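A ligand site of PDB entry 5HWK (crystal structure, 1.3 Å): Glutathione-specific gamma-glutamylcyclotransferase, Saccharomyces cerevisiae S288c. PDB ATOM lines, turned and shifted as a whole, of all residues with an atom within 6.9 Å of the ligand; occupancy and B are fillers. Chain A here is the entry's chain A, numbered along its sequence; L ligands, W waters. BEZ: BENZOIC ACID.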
ATOM      1  N   VAL A  10      -5.920  24.668  -5.670  1.00  0.00           N
ATOM      2  CA  VAL A  10      -4.990  25.198  -4.670  1.00  0.00           C
ATOM      3  C   VAL A  10      -5.243  24.476  -3.359  1.00  0.00           C
ATOM      4  O   VAL A  10      -6.369  24.488  -2.860  1.00  0.00           O
ATOM      5  CB  VAL A  10      -5.220  26.713  -4.483  1.00  0.00           C
ATOM      6  CG1 VAL A  10      -4.286  27.273  -3.366  1.00  0.00           C
ATOM      7  CG2 VAL A  10      -4.999  27.449  -5.771  1.00  0.00           C
ATOM      8  N   LEU A  11      -4.188  23.910  -2.754  1.00  0.00           N
ATOM      9  CA  LEU A  11      -4.319  23.272  -1.462  1.00  0.00           C
ATOM     10  C   LEU A  11      -4.314  24.332  -0.371  1.00  0.00           C
ATOM     11  O   LEU A  11      -3.561  25.310  -0.466  1.00  0.00           O
ATOM     12  CB  LEU A  11      -3.096  22.400  -1.197  1.00  0.00           C
ATOM     13  CG  LEU A  11      -2.908  21.133  -2.005  1.00  0.00           C
ATOM     14  CD1 LEU A  11      -1.629  20.425  -1.529  1.00  0.00           C
ATOM     15  CD2 LEU A  11      -4.134  20.300  -1.819  1.00  0.00           C
ATOM     16  N   GLY A  12      -5.184  24.158   0.602  1.00  0.00           N
ATOM     17  CA  GLY A  12      -5.085  24.953   1.816  1.00  0.00           C
ATOM     18  C   GLY A  12      -4.862  24.066   3.023  1.00  0.00           C
ATOM     19  O   GLY A  12      -5.609  23.107   3.244  1.00  0.00           O
ATOM     20  N   TYR A  13      -3.835  24.381   3.840  1.00  0.00           N
ATOM     21  CA  TYR A  13      -3.528  23.603   5.033  1.00  0.00           C
ATOM     22  C   TYR A  13      -3.410  24.507   6.256  1.00  0.00           C
ATOM     23  O   TYR A  13      -3.226  23.988   7.367  1.00  0.00           O
ATOM     24  CB  TYR A  13      -2.260  22.745   4.857  1.00  0.00           C
ATOM     25  CG  TYR A  13      -1.058  23.581   4.605  1.00  0.00           C
ATOM     26  CD1 TYR A  13      -0.291  24.053   5.650  1.00  0.00           C
ATOM     27  CD2 TYR A  13      -0.660  23.880   3.318  1.00  0.00           C
ATOM     28  CE1 TYR A  13       0.788  24.825   5.439  1.00  0.00           C
ATOM     29  CE2 TYR A  13       0.475  24.644   3.086  1.00  0.00           C
ATOM     30  CZ  TYR A  13       1.210  25.110   4.164  1.00  0.00           C
ATOM     31  OH  TYR A  13       2.338  25.865   3.945  1.00  0.00           O
ATOM     32  N   GLY A  14      -3.479  25.818   6.078  1.00  0.00           N
ATOM     33  CA  GLY A  14      -3.336  26.788   7.168  1.00  0.00           C
ATOM     34  C   GLY A  14      -4.458  27.788   7.044  1.00  0.00           C
ATOM     35  O   GLY A  14      -5.633  27.372   7.008  1.00  0.00           O
ATOM     36  N   SER A  15      -4.136  29.086   7.001  1.00  0.00           N
ATOM     37  CA  SER A  15      -5.181  30.096   6.998  1.00  0.00           C
ATOM     38  C   SER A  15      -6.043  30.060   5.763  1.00  0.00           C
ATOM     39  O   SER A  15      -7.128  30.621   5.817  1.00  0.00           O
ATOM     40  CB  SER A  15      -4.623  31.514   7.206  1.00  0.00           C
ATOM     41  OG  SER A  15      -3.777  31.893   6.146  1.00  0.00           O
ATOM     42  N   LEU A  16      -5.610  29.456   4.644  1.00  0.00           N
ATOM     43  CA  LEU A  16      -6.534  29.419   3.506  1.00  0.00           C
ATOM     44  C   LEU A  16      -7.736  28.553   3.798  1.00  0.00           C
ATOM     45  O   LEU A  16      -8.736  28.658   3.077  1.00  0.00           O
ATOM     46  CB  LEU A  16      -5.835  28.879   2.241  1.00  0.00           C
ATOM     47  CG  LEU A  16      -4.837  29.834   1.589  1.00  0.00           C
ATOM     48  CD1 LEU A  16      -3.911  29.052   0.593  1.00  0.00           C
ATOM     49  CD2 LEU A  16      -5.538  30.988   0.885  1.00  0.00           C
ATOM     50  N   ILE A  17      -7.672  27.667   4.807  1.00  0.00           N
ATOM     51  CA  ILE A  17      -8.839  26.857   5.143  1.00  0.00           C
ATOM     52  C   ILE A  17      -9.996  27.730   5.588  1.00  0.00           C
ATOM     53  O   ILE A  17     -11.140  27.562   5.161  1.00  0.00           O
ATOM     54  CB  ILE A  17      -8.496  25.822   6.236  1.00  0.00           C
ATOM     55  CG1 ILE A  17      -7.511  24.800   5.697  1.00  0.00           C
ATOM     56  CG2 ILE A  17      -9.768  25.117   6.658  1.00  0.00           C
ATOM     57  CD1 ILE A  17      -6.997  23.802   6.773  1.00  0.00           C
ATOM     58  N   TYR A  18      -9.732  28.664   6.495  1.00  0.00           N
ATOM     59  CA  TYR A  18     -10.805  29.445   7.087  1.00  0.00           C
ATOM     60  C   TYR A  18     -10.875  30.878   6.596  1.00  0.00           C
ATOM     61  O   TYR A  18     -11.863  31.567   6.897  1.00  0.00           O
ATOM     62  CB  TYR A  18     -10.733  29.437   8.613  1.00  0.00           C
ATOM     63  CG  TYR A  18      -9.397  29.892   9.135  1.00  0.00           C
ATOM     64  CD1 TYR A  18      -9.079  31.261   9.204  1.00  0.00           C
ATOM     65  CD2 TYR A  18      -8.446  28.976   9.527  1.00  0.00           C
ATOM     66  CE1 TYR A  18      -7.866  31.693   9.694  1.00  0.00           C
ATOM     67  CE2 TYR A  18      -7.224  29.416  10.036  1.00  0.00           C
ATOM     68  CZ  TYR A  18      -6.951  30.762  10.077  1.00  0.00           C
ATOM     69  OH  TYR A  18      -5.745  31.214  10.539  1.00  0.00           O
ATOM     70  N   ALA A  57       1.987  27.602  10.225  1.00  0.00           N
ATOM     71  CA  ALA A  57       2.039  26.263   9.632  1.00  0.00           C
ATOM     72  C   ALA A  57       2.846  26.213   8.331  1.00  0.00           C
ATOM     73  O   ALA A  57       2.760  27.122   7.491  1.00  0.00           O
ATOM     74  CB  ALA A  57       0.634  25.797   9.336  1.00  0.00           C
ATOM     75  N   THR A  58       3.555  25.118   8.152  1.00  0.00           N
ATOM     76  CA  THR A  58       4.124  24.777   6.837  1.00  0.00           C
ATOM     77  C   THR A  58       3.895  23.294   6.614  1.00  0.00           C
ATOM     78  O   THR A  58       3.514  22.580   7.514  1.00  0.00           O
ATOM     79  CB  THR A  58       5.606  25.222   6.764  1.00  0.00           C
ATOM     80  OG1 THR A  58       6.069  24.997   5.439  1.00  0.00           O
ATOM     81  CG2 THR A  58       6.476  24.449   7.702  1.00  0.00           C
ATOM     82  N   LEU A  59       4.092  22.833   5.384  1.00  0.00           N
ATOM     83  CA  LEU A  59       3.966  21.417   5.064  1.00  0.00           C
ATOM     84  C   LEU A  59       5.347  20.907   4.715  1.00  0.00           C
ATOM     85  O   LEU A  59       6.115  21.589   4.037  1.00  0.00           O
ATOM     86  CB  LEU A  59       3.152  21.234   3.783  1.00  0.00           C
ATOM     87  CG  LEU A  59       1.677  21.333   3.848  1.00  0.00           C
ATOM     88  CD1 LEU A  59       1.139  20.951   2.428  1.00  0.00           C
ATOM     89  CD2 LEU A  59       1.118  20.430   4.919  1.00  0.00           C
ATOM     90  N   TYR A 110      -1.855  35.370  -3.391  1.00  0.00           N
ATOM     91  CA  TYR A 110      -2.720  35.044  -2.257  1.00  0.00           C
ATOM     92  C   TYR A 110      -2.057  35.308  -0.919  1.00  0.00           C
ATOM     93  O   TYR A 110      -2.759  35.485   0.063  1.00  0.00           O
ATOM     94  CB  TYR A 110      -3.100  33.562  -2.277  1.00  0.00           C
ATOM     95  CG  TYR A 110      -4.156  33.210  -3.277  1.00  0.00           C
ATOM     96  CD1 TYR A 110      -4.905  34.189  -3.930  1.00  0.00           C
ATOM     97  CD2 TYR A 110      -4.447  31.866  -3.546  1.00  0.00           C
ATOM     98  CE1 TYR A 110      -5.910  33.840  -4.852  1.00  0.00           C
ATOM     99  CE2 TYR A 110      -5.431  31.515  -4.465  1.00  0.00           C
ATOM    100  CZ  TYR A 110      -6.154  32.490  -5.106  1.00  0.00           C
ATOM    101  OH  TYR A 110      -7.113  32.125  -6.013  1.00  0.00           O
ATOM    102  N   LEU A 111      -0.727  35.289  -0.854  1.00  0.00           N
ATOM    103  CA  LEU A 111      -0.095  35.497   0.450  1.00  0.00           C
ATOM    104  C   LEU A 111      -0.016  36.970   0.854  1.00  0.00           C
ATOM    105  O   LEU A 111       0.430  37.253   1.973  1.00  0.00           O
ATOM    106  CB  LEU A 111       1.278  34.847   0.544  1.00  0.00           C
ATOM    107  CG  LEU A 111       1.274  33.323   0.335  1.00  0.00           C
ATOM    108  CD1 LEU A 111       2.559  32.726   0.846  1.00  0.00           C
ATOM    109  CD2 LEU A 111       0.089  32.627   1.023  1.00  0.00           C
ATOM    110  N   ARG A 114      -1.747  37.510   4.147  1.00  0.00           N
ATOM    111  CA  ARG A 114      -1.585  36.510   5.200  1.00  0.00           C
ATOM    112  C   ARG A 114      -0.105  36.248   5.444  1.00  0.00           C
ATOM    113  O   ARG A 114       0.756  37.060   5.090  1.00  0.00           O
ATOM    114  CB  ARG A 114      -2.383  35.245   4.893  1.00  0.00           C
ATOM    115  CG  ARG A 114      -1.966  34.582   3.606  1.00  0.00           C
ATOM    116  CD  ARG A 114      -2.952  33.474   3.226  1.00  0.00           C
ATOM    117  NE  ARG A 114      -4.149  33.979   2.551  1.00  0.00           N
ATOM    118  CZ  ARG A 114      -5.397  33.725   2.932  1.00  0.00           C
ATOM    119  NH1 ARG A 114      -5.630  32.980   4.012  1.00  0.00           N
ATOM    120  NH2 ARG A 114      -6.414  34.195   2.203  1.00  0.00           N
ATOM    121  N   GLU A 115       0.193  35.139   6.114  1.00  0.00           N
ATOM    122  CA  GLU A 115       1.567  34.771   6.402  1.00  0.00           C
ATOM    123  C   GLU A 115       2.276  34.593   5.055  1.00  0.00           C
ATOM    124  O   GLU A 115       1.714  34.013   4.112  1.00  0.00           O
ATOM    125  CB  GLU A 115       1.545  33.433   7.133  1.00  0.00           C
ATOM    126  CG  GLU A 115       0.589  33.432   8.368  1.00  0.00           C
ATOM    127  CD  GLU A 115      -0.918  33.283   8.028  1.00  0.00           C
ATOM    128  OE1 GLU A 115      -1.366  32.606   7.050  1.00  0.00           O
ATOM    129  OE2 GLU A 115      -1.741  33.829   8.774  1.00  0.00           O
ATOM    130  N   GLN A 116       3.501  35.124   4.951  1.00  0.00           N
ATOM    131  CA  GLN A 116       4.079  35.276   3.624  1.00  0.00           C
ATOM    132  C   GLN A 116       5.596  35.121   3.605  1.00  0.00           C
ATOM    133  O   GLN A 116       6.155  34.621   2.616  1.00  0.00           O
ATOM    134  CB  GLN A 116       3.703  36.659   3.049  1.00  0.00           C
ATOM    135  CG  GLN A 116       4.174  36.867   1.614  1.00  0.00           C
ATOM    136  CD  GLN A 116       3.489  38.059   0.938  1.00  0.00           C
ATOM    137  OE1 GLN A 116       3.238  39.083   1.577  1.00  0.00           O
ATOM    138  NE2 GLN A 116       3.178  37.909  -0.361  1.00  0.00           N
ATOM    139  N   TYR A 119       7.677  31.811   2.245  1.00  0.00           N
ATOM    140  CA  TYR A 119       6.860  30.841   1.545  1.00  0.00           C
ATOM    141  C   TYR A 119       7.123  30.936   0.052  1.00  0.00           C
ATOM    142  O   TYR A 119       7.296  32.032  -0.500  1.00  0.00           O
ATOM    143  CB  TYR A 119       5.363  31.075   1.794  1.00  0.00           C
ATOM    144  CG  TYR A 119       4.899  30.674   3.174  1.00  0.00           C
ATOM    145  CD1 TYR A 119       4.466  29.361   3.447  1.00  0.00           C
ATOM    146  CD2 TYR A 119       4.925  31.590   4.229  1.00  0.00           C
ATOM    147  CE1 TYR A 119       4.021  28.998   4.716  1.00  0.00           C
ATOM    148  CE2 TYR A 119       4.472  31.238   5.502  1.00  0.00           C
ATOM    149  CZ  TYR A 119       4.031  29.946   5.746  1.00  0.00           C
ATOM    150  OH  TYR A 119       3.603  29.621   6.990  1.00  0.00           O
ATOM    151  N   VAL A 160       0.422  24.858  -4.178  1.00  0.00           N
ATOM    152  CA  VAL A 160       0.455  24.976  -2.717  1.00  0.00           C
ATOM    153  C   VAL A 160       1.584  25.913  -2.353  1.00  0.00           C
ATOM    154  O   VAL A 160       2.632  25.912  -2.983  1.00  0.00           O
ATOM    155  CB  VAL A 160       0.650  23.547  -2.121  1.00  0.00           C
ATOM    156  CG1 VAL A 160       1.979  22.912  -2.595  1.00  0.00           C
ATOM    157  CG2 VAL A 160       0.562  23.550  -0.569  1.00  0.00           C
ATOM    158  N   TYR A 161       1.396  26.706  -1.280  1.00  0.00           N
ATOM    159  CA  TYR A 161       2.460  27.551  -0.738  1.00  0.00           C
ATOM    160  C   TYR A 161       3.096  26.850   0.447  1.00  0.00           C
ATOM    161  O   TYR A 161       2.398  26.471   1.380  1.00  0.00           O
ATOM    162  CB  TYR A 161       1.881  28.891  -0.264  1.00  0.00           C
ATOM    163  CG  TYR A 161       1.699  29.914  -1.352  1.00  0.00           C
ATOM    164  CD1 TYR A 161       2.797  30.623  -1.870  1.00  0.00           C
ATOM    165  CD2 TYR A 161       0.446  30.124  -1.925  1.00  0.00           C
ATOM    166  CE1 TYR A 161       2.624  31.604  -2.857  1.00  0.00           C
ATOM    167  CE2 TYR A 161       0.262  31.097  -2.908  1.00  0.00           C
ATOM    168  CZ  TYR A 161       1.375  31.794  -3.411  1.00  0.00           C
ATOM    169  OH  TYR A 161       1.235  32.791  -4.344  1.00  0.00           O
ATOM    170  N   ILE A 162       4.424  26.731   0.423  1.00  0.00           N
ATOM    171  CA  ILE A 162       5.186  25.962   1.389  1.00  0.00           C
ATOM    172  C   ILE A 162       6.349  26.793   1.885  1.00  0.00           C
ATOM    173  O   ILE A 162       7.002  27.451   1.077  1.00  0.00           O
ATOM    174  CB  ILE A 162       5.754  24.663   0.752  1.00  0.00           C
ATOM    175  CG1 ILE A 162       4.584  23.752   0.383  1.00  0.00           C
ATOM    176  CG2 ILE A 162       6.754  23.973   1.722  1.00  0.00           C
ATOM    177  CD1 ILE A 162       4.978  22.437  -0.225  1.00  0.00           C
ATOM    178  N   GLY A 163       6.624  26.747   3.188  1.00  0.00           N
ATOM    179  CA  GLY A 163       7.919  27.208   3.714  1.00  0.00           C
ATOM    180  C   GLY A 163       8.860  26.030   3.672  1.00  0.00           C
ATOM    181  O   GLY A 163       8.714  25.132   4.489  1.00  0.00           O
ATOM    182  N   TYR A 196      -4.298  32.142  16.019  1.00  0.00           N
ATOM    183  CA  TYR A 196      -4.034  31.429  14.774  1.00  0.00           C
ATOM    184  C   TYR A 196      -4.177  29.914  14.944  1.00  0.00           C
ATOM    185  O   TYR A 196      -4.833  29.226  14.136  1.00  0.00           O
ATOM    186  CB  TYR A 196      -2.635  31.774  14.301  1.00  0.00           C
ATOM    187  CG  TYR A 196      -2.133  31.039  13.097  1.00  0.00           C
ATOM    188  CD1 TYR A 196      -1.462  29.818  13.245  1.00  0.00           C
ATOM    189  CD2 TYR A 196      -2.275  31.592  11.824  1.00  0.00           C
ATOM    190  CE1 TYR A 196      -0.972  29.135  12.133  1.00  0.00           C
ATOM    191  CE2 TYR A 196      -1.784  30.929  10.681  1.00  0.00           C
ATOM    192  CZ  TYR A 196      -1.165  29.695  10.836  1.00  0.00           C
ATOM    193  OH  TYR A 196      -0.610  29.044   9.746  1.00  0.00           O
HETATM  194  C   BEZ L   1      -2.361  27.602   3.446  1.00  0.00           C
HETATM  195  O1  BEZ L   1      -3.387  27.671   4.050  1.00  0.00           O
HETATM  196  O2  BEZ L   1      -2.173  26.567   2.787  1.00  0.00           O
HETATM  197  C1  BEZ L   1      -1.305  28.660   3.565  1.00  0.00           C
HETATM  198  C2  BEZ L   1      -0.054  28.379   3.040  1.00  0.00           C
HETATM  199  C3  BEZ L   1       0.975  29.319   3.185  1.00  0.00           C
HETATM  200  C4  BEZ L   1       0.740  30.542   3.763  1.00  0.00           C
HETATM  201  C5  BEZ L   1      -0.538  30.827   4.244  1.00  0.00           C
HETATM  202  C6  BEZ L   1      -1.572  29.897   4.166  1.00  0.00           C
HETATM  203  O   HOH W   1      -1.251  29.916   7.454  1.00  0.00           O
HETATM  204  O   HOH W   2       0.275  28.044   6.393  1.00  0.00           O
HETATM  205  O   HOH W   3      -1.198  26.625   0.080  1.00  0.00           O
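The backbone NH (N) of Tyr 13 lies within hydrogen-bond range of an oxygen (O2) of the ligand (2.9 Å).
The backbone NH (N) of Gly 14 lies within hydrogen-bond range of an oxygen (O1) of the ligand (2.7 Å).
N of Ser 15 is in hydrogen-bond range of O1 of the ligand (3.4 Å).
N of Leu 16 sits at hydrogen-bond distance from O1 of the ligand, 2.9 Å away.
Water W3 lies within hydrogen-bond range of O of Leu 11 (2.8 Å), O2 of the ligand (2.9 Å) and N of Tyr 161 (2.9 Å).
Water W1 lies within hydrogen-bond range of OH of Tyr 196, OE1 of Glu 115 and N of Ser 15.
Leu 11 touches the ligand.
Gly 12 touches the ligand (CA to O2, 3.5 Å).
Leu 111 touches the ligand (CD2 to C4, 3.5 Å).
Arg 114 touches the ligand (CD to C5, 3.7 Å).
Glu 115 touches the ligand (OE1 to C5, 3.4 Å).
CE1 of Tyr 119 touches C3 of the ligand, 3.4 Å away.
Tyr 161 touches the ligand (O to C2, 3.5 Å).
Hydrophobic or aromatic side chains within 4 Å of the ligand: Tyr 13, Leu 16, Leu 111, Tyr 119 and Tyr 161.
11 residues have an atom within 4 Å of the ligand: Leu 11, Gly 12, Tyr 13, Gly 14, Ser 15, Leu 16, Leu 111, Arg 114, Glu 115, Tyr 119 and Tyr 161.
Along chain A the residues within 4 Å of the ligand span positions 11 to 161.
The side-chain hydroxyl (OH) of Tyr 13 sits at hydrogen-bond distance from the backbone carbonyl oxygen (O) of Tyr 161.
The side-chain amide oxygen of Gln 116 lies close to the backbone carbonyl oxygen of Leu 111, 3.4 Å away.
NE of Arg 114 sits at hydrogen-bond distance from O of Tyr 110 (3.2 Å).
OH of Tyr 119 sits at hydrogen-bond distance from O of Ala 57, 2.7 Å away.
OG of Ser 15 sits at hydrogen-bond distance from NH1 of Arg 114 (3.0 Å).
The side-chain hydroxyl of Ser 15 lies within hydrogen-bond range of the side-chain carboxylate of Glu 115.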
